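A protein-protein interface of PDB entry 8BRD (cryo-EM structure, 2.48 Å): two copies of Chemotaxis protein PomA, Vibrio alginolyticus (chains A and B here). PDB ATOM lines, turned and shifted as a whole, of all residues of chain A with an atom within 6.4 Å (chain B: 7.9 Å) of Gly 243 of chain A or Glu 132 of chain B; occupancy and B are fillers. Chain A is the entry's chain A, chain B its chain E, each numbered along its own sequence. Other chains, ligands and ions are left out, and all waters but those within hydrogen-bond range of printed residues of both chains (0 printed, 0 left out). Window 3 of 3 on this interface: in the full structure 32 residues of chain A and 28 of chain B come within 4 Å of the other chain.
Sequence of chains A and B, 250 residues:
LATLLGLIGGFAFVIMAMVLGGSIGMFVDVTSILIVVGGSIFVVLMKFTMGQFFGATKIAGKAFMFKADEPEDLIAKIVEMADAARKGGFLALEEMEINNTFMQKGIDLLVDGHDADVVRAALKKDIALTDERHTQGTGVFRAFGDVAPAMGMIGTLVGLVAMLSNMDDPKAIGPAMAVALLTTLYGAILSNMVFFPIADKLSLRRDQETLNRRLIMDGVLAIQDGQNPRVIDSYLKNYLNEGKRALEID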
ATOM      1  N   TYR A 239     -18.416  11.798 -11.971  1.00  0.00           N
ATOM      2  CA  TYR A 239     -17.764  10.700 -11.265  1.00  0.00           C
ATOM      3  C   TYR A 239     -18.535  10.236 -10.037  1.00  0.00           C
ATOM      4  O   TYR A 239     -18.198   9.188  -9.478  1.00  0.00           O
ATOM      5  CB  TYR A 239     -16.348  11.105 -10.846  1.00  0.00           C
ATOM      6  CG  TYR A 239     -15.318  11.026 -11.948  1.00  0.00           C
ATOM      7  CD1 TYR A 239     -15.591  10.363 -13.136  1.00  0.00           C
ATOM      8  CD2 TYR A 239     -14.065  11.604 -11.794  1.00  0.00           C
ATOM      9  CE1 TYR A 239     -14.648  10.285 -14.144  1.00  0.00           C
ATOM     10  CE2 TYR A 239     -13.116  11.533 -12.793  1.00  0.00           C
ATOM     11  CZ  TYR A 239     -13.413  10.873 -13.967  1.00  0.00           C
ATOM     12  OH  TYR A 239     -12.472  10.798 -14.967  1.00  0.00           O
ATOM     13  N   ASN A 241     -21.623   9.245  -9.937  1.00  0.00           N
ATOM     14  CA  ASN A 241     -22.644   8.274 -10.308  1.00  0.00           C
ATOM     15  C   ASN A 241     -22.042   6.941 -10.737  1.00  0.00           C
ATOM     16  O   ASN A 241     -22.572   6.286 -11.641  1.00  0.00           O
ATOM     17  CB  ASN A 241     -23.532   8.837 -11.418  1.00  0.00           C
ATOM     18  CG  ASN A 241     -24.462   9.925 -10.923  1.00  0.00           C
ATOM     19  OD1 ASN A 241     -25.203   9.732  -9.960  1.00  0.00           O
ATOM     20  ND2 ASN A 241     -24.424  11.079 -11.577  1.00  0.00           N
ATOM     21  N   GLU A 242     -20.942   6.530 -10.114  1.00  0.00           N
ATOM     22  CA  GLU A 242     -20.304   5.252 -10.385  1.00  0.00           C
ATOM     23  C   GLU A 242     -20.139   4.471  -9.088  1.00  0.00           C
ATOM     24  O   GLU A 242     -20.251   5.011  -7.985  1.00  0.00           O
ATOM     25  CB  GLU A 242     -18.944   5.439 -11.070  1.00  0.00           C
ATOM     26  CG  GLU A 242     -19.023   5.715 -12.565  1.00  0.00           C
ATOM     27  CD  GLU A 242     -19.313   7.168 -12.883  1.00  0.00           C
ATOM     28  OE1 GLU A 242     -19.420   7.975 -11.938  1.00  0.00           O
ATOM     29  OE2 GLU A 242     -19.434   7.502 -14.081  1.00  0.00           O
ATOM     30  N   GLY A 243     -19.874   3.175  -9.237  1.00  0.00           N
ATOM     31  CA  GLY A 243     -19.689   2.328  -8.072  1.00  0.00           C
ATOM     32  C   GLY A 243     -20.992   2.092  -7.338  1.00  0.00           C
ATOM     33  O   GLY A 243     -22.038   1.828  -7.939  1.00  0.00           O
ATOM     34  N   LYS A 244     -20.929   2.192  -6.012  1.00  0.00           N
ATOM     35  CA  LYS A 244     -22.080   1.938  -5.157  1.00  0.00           C
ATOM     36  C   LYS A 244     -22.884   3.192  -4.837  1.00  0.00           C
ATOM     37  O   LYS A 244     -24.106   3.100  -4.643  1.00  0.00           O
ATOM     38  CB  LYS A 244     -21.620   1.270  -3.861  1.00  0.00           C
ATOM     39  CG  LYS A 244     -20.909  -0.052  -4.073  1.00  0.00           C
ATOM     40  CD  LYS A 244     -20.220  -0.525  -2.810  1.00  0.00           C
ATOM     41  CE  LYS A 244     -19.478  -1.828  -3.049  1.00  0.00           C
ATOM     42  NZ  LYS A 244     -18.835  -2.340  -1.809  1.00  0.00           N
ATOM     43  N   ARG A 245     -22.244   4.357  -4.783  1.00  0.00           N
ATOM     44  CA  ARG A 245     -23.021   5.583  -4.708  1.00  0.00           C
ATOM     45  C   ARG A 245     -23.936   5.748  -5.911  1.00  0.00           C
ATOM     46  O   ARG A 245     -24.984   6.388  -5.785  1.00  0.00           O
ATOM     47  CB  ARG A 245     -22.104   6.799  -4.584  1.00  0.00           C
ATOM     48  CG  ARG A 245     -21.362   6.910  -3.265  1.00  0.00           C
ATOM     49  CD  ARG A 245     -20.744   8.297  -3.126  1.00  0.00           C
ATOM     50  NE  ARG A 245     -19.727   8.645  -4.119  1.00  0.00           N
ATOM     51  CZ  ARG A 245     -18.422   8.379  -4.076  1.00  0.00           C
ATOM     52  NH1 ARG A 245     -17.905   7.526  -3.205  1.00  0.00           N
ATOM     53  NH2 ARG A 245     -17.617   8.953  -4.964  1.00  0.00           N
ATOM     54  N   ALA A 246     -23.567   5.173  -7.059  1.00  0.00           N
ATOM     55  CA  ALA A 246     -24.485   5.097  -8.190  1.00  0.00           C
ATOM     56  C   ALA A 246     -25.753   4.353  -7.808  1.00  0.00           C
ATOM     57  O   ALA A 246     -26.858   4.752  -8.193  1.00  0.00           O
ATOM     58  CB  ALA A 246     -23.809   4.409  -9.373  1.00  0.00           C
ATOM     59  N   LEU A 247     -25.616   3.268  -7.053  1.00  0.00           N
ATOM     60  CA  LEU A 247     -26.774   2.557  -6.539  1.00  0.00           C
ATOM     61  C   LEU A 247     -27.485   3.334  -5.444  1.00  0.00           C
ATOM     62  O   LEU A 247     -28.649   3.044  -5.154  1.00  0.00           O
ATOM     63  CB  LEU A 247     -26.335   1.177  -6.037  1.00  0.00           C
ATOM     64  CG  LEU A 247     -27.322   0.113  -5.549  1.00  0.00           C
ATOM     65  CD1 LEU A 247     -27.549   0.237  -4.069  1.00  0.00           C
ATOM     66  CD2 LEU A 247     -28.643   0.171  -6.299  1.00  0.00           C
ATOM     67  N   GLU A 248     -26.833   4.327  -4.842  1.00  0.00           N
ATOM     68  CA  GLU A 248     -27.493   5.152  -3.840  1.00  0.00           C
ATOM     69  C   GLU A 248     -28.372   6.260  -4.413  1.00  0.00           C
ATOM     70  O   GLU A 248     -29.349   6.641  -3.758  1.00  0.00           O
ATOM     71  CB  GLU A 248     -26.458   5.776  -2.884  1.00  0.00           C
ATOM     72  CG  GLU A 248     -26.972   6.671  -1.718  1.00  0.00           C
ATOM     73  CD  GLU A 248     -28.235   6.196  -0.973  1.00  0.00           C
ATOM     74  OE1 GLU A 248     -28.569   6.833   0.048  1.00  0.00           O
ATOM     75  OE2 GLU A 248     -28.892   5.210  -1.361  1.00  0.00           O
ATOM     76  N   GLN B  52     -27.090   3.143   1.055  1.00  0.00           N
ATOM     77  CA  GLN B  52     -26.945   2.398  -0.190  1.00  0.00           C
ATOM     78  C   GLN B  52     -27.697   1.073  -0.137  1.00  0.00           C
ATOM     79  O   GLN B  52     -28.303   0.656  -1.131  1.00  0.00           O
ATOM     80  CB  GLN B  52     -25.470   2.162  -0.481  1.00  0.00           C
ATOM     81  CG  GLN B  52     -25.231   1.168  -1.577  1.00  0.00           C
ATOM     82  CD  GLN B  52     -23.832   0.629  -1.558  1.00  0.00           C
ATOM     83  OE1 GLN B  52     -23.555  -0.414  -2.142  1.00  0.00           O
ATOM     84  NE2 GLN B  52     -22.935   1.334  -0.879  1.00  0.00           N
ATOM     85  N   ILE B  59     -34.636  -0.480  -5.237  1.00  0.00           N
ATOM     86  CA  ILE B  59     -34.655  -0.964  -6.617  1.00  0.00           C
ATOM     87  C   ILE B  59     -35.204  -2.385  -6.684  1.00  0.00           C
ATOM     88  O   ILE B  59     -35.881  -2.744  -7.653  1.00  0.00           O
ATOM     89  CB  ILE B  59     -33.273  -0.862  -7.292  1.00  0.00           C
ATOM     90  CG1 ILE B  59     -32.312  -1.932  -6.778  1.00  0.00           C
ATOM     91  CG2 ILE B  59     -32.692   0.527  -7.111  1.00  0.00           C
ATOM     92  CD1 ILE B  59     -31.114  -2.135  -7.663  1.00  0.00           C
ATOM     93  N   LYS B 125     -25.439   7.607 -20.942  1.00  0.00           N
ATOM     94  CA  LYS B 125     -25.128   7.809 -19.531  1.00  0.00           C
ATOM     95  C   LYS B 125     -26.221   7.226 -18.644  1.00  0.00           C
ATOM     96  O   LYS B 125     -25.936   6.566 -17.640  1.00  0.00           O
ATOM     97  CB  LYS B 125     -24.937   9.299 -19.250  1.00  0.00           C
ATOM     98  CG  LYS B 125     -24.734   9.642 -17.784  1.00  0.00           C
ATOM     99  CD  LYS B 125     -25.662  10.764 -17.349  1.00  0.00           C
ATOM    100  CE  LYS B 125     -25.038  11.595 -16.240  1.00  0.00           C
ATOM    101  NZ  LYS B 125     -24.250  10.758 -15.295  1.00  0.00           N
ATOM    102  N   ASP B 126     -27.485   7.460 -19.007  1.00  0.00           N
ATOM    103  CA  ASP B 126     -28.583   6.890 -18.232  1.00  0.00           C
ATOM    104  C   ASP B 126     -28.573   5.366 -18.294  1.00  0.00           C
ATOM    105  O   ASP B 126     -28.849   4.694 -17.293  1.00  0.00           O
ATOM    106  CB  ASP B 126     -29.923   7.433 -18.719  1.00  0.00           C
ATOM    107  CG  ASP B 126     -30.988   7.405 -17.640  1.00  0.00           C
ATOM    108  OD1 ASP B 126     -30.810   6.668 -16.648  1.00  0.00           O
ATOM    109  OD2 ASP B 126     -32.007   8.111 -17.784  1.00  0.00           O
ATOM    110  N   ILE B 127     -28.269   4.804 -19.466  1.00  0.00           N
ATOM    111  CA  ILE B 127     -28.205   3.351 -19.604  1.00  0.00           C
ATOM    112  C   ILE B 127     -27.135   2.781 -18.685  1.00  0.00           C
ATOM    113  O   ILE B 127     -27.366   1.807 -17.956  1.00  0.00           O
ATOM    114  CB  ILE B 127     -27.943   2.961 -21.071  1.00  0.00           C
ATOM    115  CG1 ILE B 127     -29.162   3.270 -21.935  1.00  0.00           C
ATOM    116  CG2 ILE B 127     -27.569   1.491 -21.175  1.00  0.00           C
ATOM    117  CD1 ILE B 127     -28.925   3.059 -23.411  1.00  0.00           C
ATOM    118  N   ALA B 128     -25.944   3.383 -18.709  1.00  0.00           N
ATOM    119  CA  ALA B 128     -24.859   2.912 -17.855  1.00  0.00           C
ATOM    120  C   ALA B 128     -25.219   3.059 -16.383  1.00  0.00           C
ATOM    121  O   ALA B 128     -24.913   2.180 -15.573  1.00  0.00           O
ATOM    122  CB  ALA B 128     -23.571   3.668 -18.173  1.00  0.00           C
ATOM    123  N   LEU B 129     -25.880   4.162 -16.023  1.00  0.00           N
ATOM    124  CA  LEU B 129     -26.262   4.371 -14.631  1.00  0.00           C
ATOM    125  C   LEU B 129     -27.247   3.308 -14.161  1.00  0.00           C
ATOM    126  O   LEU B 129     -27.088   2.737 -13.077  1.00  0.00           O
ATOM    127  CB  LEU B 129     -26.853   5.769 -14.457  1.00  0.00           C
ATOM    128  CG  LEU B 129     -27.574   6.024 -13.135  1.00  0.00           C
ATOM    129  CD1 LEU B 129     -26.577   6.055 -11.990  1.00  0.00           C
ATOM    130  CD2 LEU B 129     -28.360   7.319 -13.200  1.00  0.00           C
ATOM    131  N   THR B 130     -28.279   3.029 -14.964  1.00  0.00           N
ATOM    132  CA  THR B 130     -29.261   2.020 -14.574  1.00  0.00           C
ATOM    133  C   THR B 130     -28.637   0.631 -14.512  1.00  0.00           C
ATOM    134  O   THR B 130     -28.943  -0.155 -13.604  1.00  0.00           O
ATOM    135  CB  THR B 130     -30.447   2.028 -15.537  1.00  0.00           C
ATOM    136  OG1 THR B 130     -29.991   1.709 -16.857  1.00  0.00           O
ATOM    137  CG2 THR B 130     -31.119   3.391 -15.542  1.00  0.00           C
ATOM    138  N   ASP B 131     -27.761   0.312 -15.468  1.00  0.00           N
ATOM    139  CA  ASP B 131     -27.064  -0.968 -15.427  1.00  0.00           C
ATOM    140  C   ASP B 131     -26.229  -1.091 -14.160  1.00  0.00           C
ATOM    141  O   ASP B 131     -26.224  -2.143 -13.512  1.00  0.00           O
ATOM    142  CB  ASP B 131     -26.183  -1.124 -16.664  1.00  0.00           C
ATOM    143  CG  ASP B 131     -25.497  -2.473 -16.723  1.00  0.00           C
ATOM    144  OD1 ASP B 131     -26.155  -3.456 -17.117  1.00  0.00           O
ATOM    145  OD2 ASP B 131     -24.302  -2.553 -16.367  1.00  0.00           O
ATOM    146  N   GLU B 132     -25.528  -0.018 -13.786  1.00  0.00           N
ATOM    147  CA  GLU B 132     -24.727  -0.042 -12.570  1.00  0.00           C
ATOM    148  C   GLU B 132     -25.600  -0.204 -11.333  1.00  0.00           C
ATOM    149  O   GLU B 132     -25.246  -0.951 -10.416  1.00  0.00           O
ATOM    150  CB  GLU B 132     -23.887   1.229 -12.466  1.00  0.00           C
ATOM    151  CG  GLU B 132     -22.671   1.102 -11.560  1.00  0.00           C
ATOM    152  CD  GLU B 132     -21.724  -0.001 -11.994  1.00  0.00           C
ATOM    153  OE1 GLU B 132     -21.649  -0.288 -13.208  1.00  0.00           O
ATOM    154  OE2 GLU B 132     -21.050  -0.584 -11.119  1.00  0.00           O
ATOM    155  N   ARG B 133     -26.736   0.494 -11.281  1.00  0.00           N
ATOM    156  CA  ARG B 133     -27.614   0.371 -10.122  1.00  0.00           C
ATOM    157  C   ARG B 133     -28.125  -1.054  -9.971  1.00  0.00           C
ATOM    158  O   ARG B 133     -28.120  -1.612  -8.865  1.00  0.00           O
ATOM    159  CB  ARG B 133     -28.786   1.344 -10.233  1.00  0.00           C
ATOM    160  CG  ARG B 133     -28.391   2.802 -10.303  1.00  0.00           C
ATOM    161  CD  ARG B 133     -29.611   3.692 -10.196  1.00  0.00           C
ATOM    162  NE  ARG B 133     -30.285   3.520  -8.917  1.00  0.00           N
ATOM    163  CZ  ARG B 133     -31.521   3.926  -8.660  1.00  0.00           C
ATOM    164  NH1 ARG B 133     -32.262   4.513  -9.584  1.00  0.00           N
ATOM    165  NH2 ARG B 133     -32.023   3.739  -7.444  1.00  0.00           N
ATOM    166  N   HIS B 134     -28.567  -1.665 -11.073  1.00  0.00           N
ATOM    167  CA  HIS B 134     -29.054  -3.037 -10.990  1.00  0.00           C
ATOM    168  C   HIS B 134     -27.936  -4.005 -10.620  1.00  0.00           C
ATOM    169  O   HIS B 134     -28.145  -4.919  -9.813  1.00  0.00           O
ATOM    170  CB  HIS B 134     -29.718  -3.442 -12.301  1.00  0.00           C
ATOM    171  CG  HIS B 134     -31.138  -2.990 -12.412  1.00  0.00           C
ATOM    172  ND1 HIS B 134     -31.519  -1.908 -13.173  1.00  0.00           N
ATOM    173  CD2 HIS B 134     -32.270  -3.469 -11.845  1.00  0.00           C
ATOM    174  CE1 HIS B 134     -32.827  -1.742 -13.075  1.00  0.00           C
ATOM    175  NE2 HIS B 134     -33.305  -2.678 -12.277  1.00  0.00           N
ATOM    176  N   THR B 135     -26.743  -3.817 -11.186  1.00  0.00           N
ATOM    177  CA  THR B 135     -25.624  -4.688 -10.844  1.00  0.00           C
ATOM    178  C   THR B 135     -25.251  -4.560  -9.373  1.00  0.00           C
ATOM    179  O   THR B 135     -24.935  -5.557  -8.716  1.00  0.00           O
ATOM    180  CB  THR B 135     -24.424  -4.371 -11.734  1.00  0.00           C
ATOM    181  OG1 THR B 135     -24.805  -4.505 -13.109  1.00  0.00           O
ATOM    182  CG2 THR B 135     -23.279  -5.325 -11.449  1.00  0.00           C
ATOM    183  N   GLN B 136     -25.298  -3.344  -8.830  1.00  0.00           N
ATOM    184  CA  GLN B 136     -24.932  -3.154  -7.432  1.00  0.00           C
ATOM    185  C   GLN B 136     -25.996  -3.712  -6.494  1.00  0.00           C
ATOM    186  O   GLN B 136     -25.666  -4.254  -5.433  1.00  0.00           O
ATOM    187  CB  GLN B 136     -24.678  -1.676  -7.150  1.00  0.00           C
ATOM    188  CG  GLN B 136     -23.429  -1.118  -7.810  1.00  0.00           C
ATOM    189  CD  GLN B 136     -22.186  -1.922  -7.492  1.00  0.00           C
ATOM    190  OE1 GLN B 136     -22.017  -2.411  -6.375  1.00  0.00           O
ATOM    191  NE2 GLN B 136     -21.307  -2.064  -8.477  1.00  0.00           N
ATOM    192  N   GLY B 137     -27.276  -3.586  -6.854  1.00  0.00           N
ATOM    193  CA  GLY B 137     -28.311  -4.243  -6.068  1.00  0.00           C
ATOM    194  C   GLY B 137     -28.172  -5.754  -6.084  1.00  0.00           C
ATOM    195  O   GLY B 137     -28.329  -6.419  -5.053  1.00  0.00           O
ATOM    196  N   THR B 138     -27.863  -6.313  -7.256  1.00  0.00           N
ATOM    197  CA  THR B 138     -27.578  -7.739  -7.354  1.00  0.00           C
ATOM    198  C   THR B 138     -26.400  -8.117  -6.469  1.00  0.00           C
ATOM    199  O   THR B 138     -26.423  -9.154  -5.801  1.00  0.00           O
ATOM    200  CB  THR B 138     -27.303  -8.115  -8.811  1.00  0.00           C
ATOM    201  OG1 THR B 138     -28.535  -8.138  -9.540  1.00  0.00           O
ATOM    202  CG2 THR B 138     -26.641  -9.476  -8.909  1.00  0.00           C
ATOM    203  N   GLY B 139     -25.362  -7.280  -6.445  1.00  0.00           N
ATOM    204  CA  GLY B 139     -24.225  -7.546  -5.578  1.00  0.00           C
ATOM    205  C   GLY B 139     -24.584  -7.514  -4.104  1.00  0.00           C
ATOM    206  O   GLY B 139     -24.112  -8.341  -3.326  1.00  0.00           O
ATOM    207  N   ARG B 206     -32.490  -6.122 -14.951  1.00  0.00           N
ATOM    208  CA  ARG B 206     -31.408  -5.398 -15.609  1.00  0.00           C
ATOM    209  C   ARG B 206     -31.338  -5.730 -17.090  1.00  0.00           C
ATOM    210  O   ARG B 206     -31.114  -4.844 -17.919  1.00  0.00           O
ATOM    211  CB  ARG B 206     -30.076  -5.727 -14.938  1.00  0.00           C
ATOM    212  CG  ARG B 206     -28.888  -5.027 -15.562  1.00  0.00           C
ATOM    213  CD  ARG B 206     -27.606  -5.339 -14.816  1.00  0.00           C
ATOM    214  NE  ARG B 206     -26.781  -6.295 -15.542  1.00  0.00           N
ATOM    215  CZ  ARG B 206     -26.302  -7.417 -15.021  1.00  0.00           C
ATOM    216  NH1 ARG B 206     -26.525  -7.742 -13.758  1.00  0.00           N
ATOM    217  NH2 ARG B 206     -25.578  -8.228 -15.785  1.00  0.00           N
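No position is printed for both chains.
Of the 12 pairs that touch across the chains among the printed residues, none has its exchanged pair printed and touching as well.
Glu 132 of chain B touches just one residue of chain A: Gly 243 (3.7 Å).
Printed residues of chain A within 4 Å of Lys 125 of chain B: Asn 241.
Printed residues of chain A within 4 Å of Gln 136 of chain B: Gly 243 (3.3 Å), Lys 244 (3.5 Å) and Leu 247 (3.5 Å).
The nearest residue of chain B that does not touch Gly 243 of chain A is Arg 133 of chain B (5.9 Å).
The nearest printed residue of chain B that does not touch Lys 244 of chain A is Glu 132 of chain B (5.8 Å).
Hydrophobic or aromatic side chains of chain B within 4 Å of the printed part of chain A: Ile 59.
Along chain B the printed residues that touch a printed residue of chain A span positions 52 to 137.
Among the printed residues, 12 pairs touch across the chains.
NZ of Lys 125 of chain B touches ND2 of Asn 241 of chain A, at 3.7 Å.
CG of Glu 132 of chain B touches O of Gly 243 of chain A, 3.7 Å away.
O of Gly 243 of chain A touches CG of Gln 136 of chain B, 3.3 Å away.
OE1 of Gln 52 of chain B touches CB of Lys 244 of chain A, 3.1 Å away.
Arg 133 of chain B touches Ala 246 of chain A.
Gln 52 of chain B touches Leu 247 of chain A (O to CD1, 3.1 Å).
Ile 59 of chain B touches Leu 247 of chain A.
O of Arg 133 of chain B touches CD2 of Leu 247 of chain A, at 3.2 Å.
Gly 137 of chain B touches Leu 247 of chain A.
Gln 52 of chain B touches Glu 248 of chain A.
OE2 of Glu 132 of chain B sits at hydrogen-bond distance from NE2 of Gln 136 of chain B (3.0 Å).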
